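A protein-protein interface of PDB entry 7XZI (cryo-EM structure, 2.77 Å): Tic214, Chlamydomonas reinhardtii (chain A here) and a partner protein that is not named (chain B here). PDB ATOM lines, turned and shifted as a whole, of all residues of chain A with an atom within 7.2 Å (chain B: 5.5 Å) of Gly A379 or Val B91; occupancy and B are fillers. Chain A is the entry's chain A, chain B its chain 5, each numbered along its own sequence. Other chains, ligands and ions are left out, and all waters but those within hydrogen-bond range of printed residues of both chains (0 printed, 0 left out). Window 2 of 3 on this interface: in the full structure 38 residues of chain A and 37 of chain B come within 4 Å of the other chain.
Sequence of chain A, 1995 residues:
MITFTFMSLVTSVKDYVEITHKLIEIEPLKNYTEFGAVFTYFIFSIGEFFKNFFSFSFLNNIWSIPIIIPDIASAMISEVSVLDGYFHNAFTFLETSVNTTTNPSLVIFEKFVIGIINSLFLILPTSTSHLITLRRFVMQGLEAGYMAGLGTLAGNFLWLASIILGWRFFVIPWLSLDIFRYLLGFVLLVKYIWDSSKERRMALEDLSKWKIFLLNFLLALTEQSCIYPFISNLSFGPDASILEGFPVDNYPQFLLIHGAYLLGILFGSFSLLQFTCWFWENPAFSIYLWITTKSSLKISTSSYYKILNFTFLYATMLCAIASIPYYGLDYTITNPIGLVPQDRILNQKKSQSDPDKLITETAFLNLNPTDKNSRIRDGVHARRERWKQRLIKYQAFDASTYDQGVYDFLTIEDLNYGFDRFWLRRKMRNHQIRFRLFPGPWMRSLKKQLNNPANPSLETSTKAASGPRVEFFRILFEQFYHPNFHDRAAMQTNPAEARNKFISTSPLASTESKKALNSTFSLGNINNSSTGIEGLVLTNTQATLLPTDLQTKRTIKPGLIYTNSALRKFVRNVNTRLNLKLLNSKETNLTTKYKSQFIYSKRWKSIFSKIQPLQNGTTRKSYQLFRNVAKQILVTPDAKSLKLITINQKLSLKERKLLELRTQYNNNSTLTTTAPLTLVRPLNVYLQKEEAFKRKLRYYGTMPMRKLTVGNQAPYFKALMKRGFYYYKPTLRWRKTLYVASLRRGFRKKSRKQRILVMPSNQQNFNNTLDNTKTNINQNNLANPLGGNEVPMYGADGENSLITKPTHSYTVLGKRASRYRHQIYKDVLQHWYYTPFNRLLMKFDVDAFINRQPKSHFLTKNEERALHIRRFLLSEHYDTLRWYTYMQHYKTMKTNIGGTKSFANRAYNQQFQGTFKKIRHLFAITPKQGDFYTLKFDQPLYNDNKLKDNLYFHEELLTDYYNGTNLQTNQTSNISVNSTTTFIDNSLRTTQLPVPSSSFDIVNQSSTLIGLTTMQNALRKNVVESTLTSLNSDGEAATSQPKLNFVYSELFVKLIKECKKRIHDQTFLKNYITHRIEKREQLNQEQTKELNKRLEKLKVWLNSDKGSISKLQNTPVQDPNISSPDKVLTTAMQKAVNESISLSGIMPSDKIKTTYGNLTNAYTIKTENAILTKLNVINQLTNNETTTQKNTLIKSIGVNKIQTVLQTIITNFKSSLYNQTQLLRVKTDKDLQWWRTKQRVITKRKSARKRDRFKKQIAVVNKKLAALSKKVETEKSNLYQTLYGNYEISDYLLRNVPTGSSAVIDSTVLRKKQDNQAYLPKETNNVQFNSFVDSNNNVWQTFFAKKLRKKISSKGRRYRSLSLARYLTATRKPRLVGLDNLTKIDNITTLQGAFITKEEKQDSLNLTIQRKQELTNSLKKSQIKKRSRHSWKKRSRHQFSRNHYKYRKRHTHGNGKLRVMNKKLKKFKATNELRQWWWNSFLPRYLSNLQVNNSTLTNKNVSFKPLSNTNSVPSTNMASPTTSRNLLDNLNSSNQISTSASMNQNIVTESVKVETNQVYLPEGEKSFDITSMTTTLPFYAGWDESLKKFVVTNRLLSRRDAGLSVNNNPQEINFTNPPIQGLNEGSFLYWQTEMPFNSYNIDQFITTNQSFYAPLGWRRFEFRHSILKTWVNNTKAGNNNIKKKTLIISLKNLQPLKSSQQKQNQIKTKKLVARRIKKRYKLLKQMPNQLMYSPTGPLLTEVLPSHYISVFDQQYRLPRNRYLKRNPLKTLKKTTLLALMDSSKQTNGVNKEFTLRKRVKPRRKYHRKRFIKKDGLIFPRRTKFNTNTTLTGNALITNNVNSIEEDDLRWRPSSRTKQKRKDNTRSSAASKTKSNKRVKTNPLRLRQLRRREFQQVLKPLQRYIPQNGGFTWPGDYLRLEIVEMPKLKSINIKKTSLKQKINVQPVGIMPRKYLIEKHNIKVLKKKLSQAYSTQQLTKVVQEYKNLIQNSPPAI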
ATOM      1  N   ILE A 376     -16.917   5.939 -27.847  1.00  0.00           N
ATOM      2  CA  ILE A 376     -17.681   6.341 -26.675  1.00  0.00           C
ATOM      3  C   ILE A 376     -18.650   5.253 -26.235  1.00  0.00           C
ATOM      4  O   ILE A 376     -19.540   5.514 -25.418  1.00  0.00           O
ATOM      5  CB  ILE A 376     -18.421   7.665 -26.912  1.00  0.00           C
ATOM      6  CG1 ILE A 376     -19.399   7.526 -28.080  1.00  0.00           C
ATOM      7  CG2 ILE A 376     -17.431   8.788 -27.163  1.00  0.00           C
ATOM      8  N   ARG A 377     -18.507   4.040 -26.760  1.00  0.00           N
ATOM      9  CA  ARG A 377     -19.331   2.933 -26.303  1.00  0.00           C
ATOM     10  C   ARG A 377     -18.995   2.588 -24.856  1.00  0.00           C
ATOM     11  O   ARG A 377     -17.891   2.850 -24.371  1.00  0.00           O
ATOM     12  CB  ARG A 377     -19.135   1.715 -27.208  1.00  0.00           C
ATOM     13  CG  ARG A 377     -19.661   1.916 -28.618  1.00  0.00           C
ATOM     14  CD  ARG A 377     -19.312   0.747 -29.519  1.00  0.00           C
ATOM     15  NE  ARG A 377     -17.876   0.624 -29.718  1.00  0.00           N
ATOM     16  CZ  ARG A 377     -17.304  -0.264 -30.523  1.00  0.00           C
ATOM     17  NH1 ARG A 377     -18.025  -1.125 -31.223  1.00  0.00           N
ATOM     18  NH2 ARG A 377     -15.980  -0.286 -30.630  1.00  0.00           N
ATOM     19  N   ASP A 378     -19.973   2.016 -24.160  1.00  0.00           N
ATOM     20  CA  ASP A 378     -19.822   1.736 -22.738  1.00  0.00           C
ATOM     21  C   ASP A 378     -18.711   0.721 -22.498  1.00  0.00           C
ATOM     22  O   ASP A 378     -18.641  -0.311 -23.172  1.00  0.00           O
ATOM     23  CB  ASP A 378     -21.138   1.222 -22.160  1.00  0.00           C
ATOM     24  N   GLY A 379     -17.844   1.019 -21.533  1.00  0.00           N
ATOM     25  CA  GLY A 379     -16.812   0.082 -21.131  1.00  0.00           C
ATOM     26  C   GLY A 379     -15.726  -0.170 -22.150  1.00  0.00           C
ATOM     27  O   GLY A 379     -15.283  -1.313 -22.296  1.00  0.00           O
ATOM     28  N   VAL A 380     -15.287   0.858 -22.869  1.00  0.00           N
ATOM     29  CA  VAL A 380     -14.221   0.712 -23.850  1.00  0.00           C
ATOM     30  C   VAL A 380     -12.907   1.294 -23.344  1.00  0.00           C
ATOM     31  O   VAL A 380     -11.845   0.720 -23.585  1.00  0.00           O
ATOM     32  CB  VAL A 380     -14.637   1.351 -25.192  1.00  0.00           C
ATOM     33  CG1 VAL A 380     -13.505   1.253 -26.200  1.00  0.00           C
ATOM     34  CG2 VAL A 380     -15.881   0.672 -25.732  1.00  0.00           C
ATOM     35  N   HIS A 381     -12.974   2.422 -22.630  1.00  0.00           N
ATOM     36  CA  HIS A 381     -11.814   3.141 -22.103  1.00  0.00           C
ATOM     37  C   HIS A 381     -10.704   3.249 -23.141  1.00  0.00           C
ATOM     38  O   HIS A 381      -9.594   2.745 -22.941  1.00  0.00           O
ATOM     39  CB  HIS A 381     -11.298   2.508 -20.796  1.00  0.00           C
ATOM     40  CG  HIS A 381     -11.139   1.018 -20.843  1.00  0.00           C
ATOM     41  ND1 HIS A 381     -12.152   0.152 -20.494  1.00  0.00           N
ATOM     42  CD2 HIS A 381     -10.081   0.243 -21.179  1.00  0.00           C
ATOM     43  CE1 HIS A 381     -11.728  -1.093 -20.624  1.00  0.00           C
ATOM     44  NE2 HIS A 381     -10.474  -1.064 -21.039  1.00  0.00           N
ATOM     45  N   ALA A 382     -11.005   3.918 -24.254  1.00  0.00           N
ATOM     46  CA  ALA A 382     -10.053   4.122 -25.338  1.00  0.00           C
ATOM     47  C   ALA A 382      -9.263   5.403 -25.112  1.00  0.00           C
ATOM     48  O   ALA A 382      -9.308   5.980 -24.020  1.00  0.00           O
ATOM     49  CB  ALA A 382     -10.773   4.170 -26.687  1.00  0.00           C
ATOM     50  N   LEU B  87     -14.547  -6.831 -30.729  1.00  0.00           N
ATOM     51  CA  LEU B  87     -14.253  -6.008 -29.557  1.00  0.00           C
ATOM     52  C   LEU B  87     -15.451  -5.919 -28.619  1.00  0.00           C
ATOM     53  O   LEU B  87     -15.300  -6.029 -27.394  1.00  0.00           O
ATOM     54  CB  LEU B  87     -13.812  -4.613 -29.998  1.00  0.00           C
ATOM     55  CG  LEU B  87     -13.382  -3.646 -28.894  1.00  0.00           C
ATOM     56  CD1 LEU B  87     -12.192  -4.214 -28.145  1.00  0.00           C
ATOM     57  CD2 LEU B  87     -13.053  -2.276 -29.467  1.00  0.00           C
ATOM     58  N   ASN B  88     -16.651  -5.722 -29.173  1.00  0.00           N
ATOM     59  CA  ASN B  88     -17.823  -5.469 -28.342  1.00  0.00           C
ATOM     60  C   ASN B  88     -18.196  -6.675 -27.487  1.00  0.00           C
ATOM     61  O   ASN B  88     -18.706  -6.504 -26.378  1.00  0.00           O
ATOM     62  CB  ASN B  88     -19.005  -5.051 -29.215  1.00  0.00           C
ATOM     63  CG  ASN B  88     -19.211  -5.973 -30.399  1.00  0.00           C
ATOM     64  OD1 ASN B  88     -18.730  -7.106 -30.414  1.00  0.00           O
ATOM     65  ND2 ASN B  88     -19.931  -5.489 -31.405  1.00  0.00           N
ATOM     66  N   TRP B  89     -17.961  -7.892 -27.979  1.00  0.00           N
ATOM     67  CA  TRP B  89     -18.275  -9.078 -27.186  1.00  0.00           C
ATOM     68  C   TRP B  89     -17.416  -9.140 -25.927  1.00  0.00           C
ATOM     69  O   TRP B  89     -17.920  -9.375 -24.821  1.00  0.00           O
ATOM     70  CB  TRP B  89     -18.089 -10.333 -28.038  1.00  0.00           C
ATOM     71  CG  TRP B  89     -18.566 -11.589 -27.384  1.00  0.00           C
ATOM     72  CD1 TRP B  89     -19.820 -12.120 -27.447  1.00  0.00           C
ATOM     73  CD2 TRP B  89     -17.791 -12.480 -26.576  1.00  0.00           C
ATOM     74  NE1 TRP B  89     -19.877 -13.287 -26.723  1.00  0.00           N
ATOM     75  CE2 TRP B  89     -18.644 -13.530 -26.178  1.00  0.00           C
ATOM     76  CE3 TRP B  89     -16.462 -12.492 -26.147  1.00  0.00           C
ATOM     77  CZ2 TRP B  89     -18.209 -14.580 -25.373  1.00  0.00           C
ATOM     78  CZ3 TRP B  89     -16.032 -13.535 -25.349  1.00  0.00           C
ATOM     79  CH2 TRP B  89     -16.902 -14.565 -24.970  1.00  0.00           C
ATOM     80  N   PHE B  90     -16.107  -8.917 -26.080  1.00  0.00           N
ATOM     81  CA  PHE B  90     -15.222  -8.867 -24.922  1.00  0.00           C
ATOM     82  C   PHE B  90     -15.583  -7.706 -24.008  1.00  0.00           C
ATOM     83  O   PHE B  90     -15.490  -7.822 -22.780  1.00  0.00           O
ATOM     84  CB  PHE B  90     -13.765  -8.763 -25.371  1.00  0.00           C
ATOM     85  CG  PHE B  90     -13.207 -10.040 -25.930  1.00  0.00           C
ATOM     86  CD1 PHE B  90     -12.815 -11.065 -25.088  1.00  0.00           C
ATOM     87  CD2 PHE B  90     -13.066 -10.212 -27.296  1.00  0.00           C
ATOM     88  CE1 PHE B  90     -12.298 -12.240 -25.599  1.00  0.00           C
ATOM     89  CE2 PHE B  90     -12.552 -11.383 -27.813  1.00  0.00           C
ATOM     90  CZ  PHE B  90     -12.168 -12.399 -26.963  1.00  0.00           C
ATOM     91  N   VAL B  91     -15.992  -6.575 -24.586  1.00  0.00           N
ATOM     92  CA  VAL B  91     -16.400  -5.431 -23.775  1.00  0.00           C
ATOM     93  C   VAL B  91     -17.614  -5.781 -22.920  1.00  0.00           C
ATOM     94  O   VAL B  91     -17.668  -5.455 -21.727  1.00  0.00           O
ATOM     95  CB  VAL B  91     -16.673  -4.214 -24.679  1.00  0.00           C
ATOM     96  CG1 VAL B  91     -17.442  -3.152 -23.921  1.00  0.00           C
ATOM     97  CG2 VAL B  91     -15.368  -3.650 -25.214  1.00  0.00           C
ATOM     98  N   GLN B  92     -18.605  -6.448 -23.515  1.00  0.00           N
ATOM     99  CA  GLN B  92     -19.796  -6.838 -22.767  1.00  0.00           C
ATOM    100  C   GLN B  92     -19.462  -7.853 -21.683  1.00  0.00           C
ATOM    101  O   GLN B  92     -20.002  -7.787 -20.572  1.00  0.00           O
ATOM    102  CB  GLN B  92     -20.858  -7.395 -23.714  1.00  0.00           C
ATOM    103  CG  GLN B  92     -21.404  -6.385 -24.711  1.00  0.00           C
ATOM    104  CD  GLN B  92     -22.130  -5.232 -24.045  1.00  0.00           C
ATOM    105  OE1 GLN B  92     -22.655  -5.364 -22.938  1.00  0.00           O
ATOM    106  NE2 GLN B  92     -22.164  -4.089 -24.720  1.00  0.00           N
ATOM    107  N   THR B  93     -18.582  -8.810 -21.988  1.00  0.00           N
ATOM    108  CA  THR B  93     -18.163  -9.771 -20.969  1.00  0.00           C
ATOM    109  C   THR B  93     -17.448  -9.074 -19.816  1.00  0.00           C
ATOM    110  O   THR B  93     -17.680  -9.394 -18.642  1.00  0.00           O
ATOM    111  CB  THR B  93     -17.268 -10.841 -21.592  1.00  0.00           C
ATOM    112  OG1 THR B  93     -17.988 -11.520 -22.628  1.00  0.00           O
ATOM    113  CG2 THR B  93     -16.835 -11.852 -20.542  1.00  0.00           C
ATOM    114  N   GLU B  94     -16.577  -8.112 -20.130  1.00  0.00           N
ATOM    115  CA  GLU B  94     -15.886  -7.357 -19.090  1.00  0.00           C
ATOM    116  C   GLU B  94     -16.865  -6.554 -18.245  1.00  0.00           C
ATOM    117  O   GLU B  94     -16.707  -6.464 -17.023  1.00  0.00           O
ATOM    118  CB  GLU B  94     -14.837  -6.439 -19.719  1.00  0.00           C
ATOM    119  CG  GLU B  94     -14.172  -5.486 -18.739  1.00  0.00           C
ATOM    120  CD  GLU B  94     -13.159  -4.575 -19.407  1.00  0.00           C
ATOM    121  OE1 GLU B  94     -12.569  -4.984 -20.429  1.00  0.00           O
ATOM    122  OE2 GLU B  94     -12.957  -3.447 -18.911  1.00  0.00           O
ATOM    123  N   LEU B  95     -17.876  -5.952 -18.877  1.00  0.00           N
ATOM    124  CA  LEU B  95     -18.881  -5.211 -18.119  1.00  0.00           C
ATOM    125  C   LEU B  95     -19.688  -6.136 -17.216  1.00  0.00           C
ATOM    126  O   LEU B  95     -20.017  -5.774 -16.081  1.00  0.00           O
ATOM    127  CB  LEU B  95     -19.805  -4.446 -19.068  1.00  0.00           C
ATOM    128  CG  LEU B  95     -19.281  -3.105 -19.584  1.00  0.00           C
ATOM    129  CD1 LEU B  95     -20.323  -2.419 -20.453  1.00  0.00           C
ATOM    130  CD2 LEU B  95     -18.877  -2.212 -18.423  1.00  0.00           C
ATOM    131  N   LEU B  96     -20.029  -7.330 -17.708  1.00  0.00           N
ATOM    132  CA  LEU B  96     -20.727  -8.301 -16.870  1.00  0.00           C
ATOM    133  C   LEU B  96     -19.873  -8.712 -15.679  1.00  0.00           C
ATOM    134  O   LEU B  96     -20.383  -8.884 -14.567  1.00  0.00           O
ATOM    135  CB  LEU B  96     -21.123  -9.527 -17.697  1.00  0.00           C
ATOM    136  CG  LEU B  96     -22.581  -9.604 -18.159  1.00  0.00           C
ATOM    137  CD1 LEU B  96     -22.932  -8.429 -19.060  1.00  0.00           C
ATOM    138  CD2 LEU B  96     -22.859 -10.926 -18.860  1.00  0.00           C
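Among the printed residues, pairs that only touch across the chains: Arg A377 with Leu B87, Asp A378 with Val B91, Asp A378 with Leu B95, Gly A379 with Val B91 and His A381 with Glu B94.
Hydrophobic or aromatic side chains of chain A within 4 Å of the printed part of chain B: His A381.
Of the 10 printed residues of chain B, 4 touch a printed residue of chain A.
Printed residues of chain B that touch a printed residue of chain A: Leu B87, Val B91, Glu B94 and Leu B95.
Hydrophobic or aromatic side chains of chain B within 4 Å of the printed part of chain A: Leu B87, Val B91 and Leu B95.
Among the printed residues, no Asp or Glu carboxylate lies within 4 Å of a Lys or Arg side-chain nitrogen of the other chain.
Printed residues of chain B within 4 Å of Arg A377: Leu B87 (3.7 Å).
Gly A379 touches just one residue of chain B: Val B91 (3.3 Å).
Val B91 touches two residues of chain A.
Gln B92 touches none of the printed residues of chain A.
Printed residues of chain A within 4 Å of Glu B94: His A381.
Of the printed residues of chain A, Leu B95 touches Asp A378 (3.8 Å).
The nearest residue of chain B that does not touch Gly A379 is Leu B95 (4.1 Å).
The nearest residue of chain A that does not touch Val B91 is Val A380 (4.4 Å).
The nearest printed residue of chain A that does not touch Leu B95 is Gly A379 (4.1 Å).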
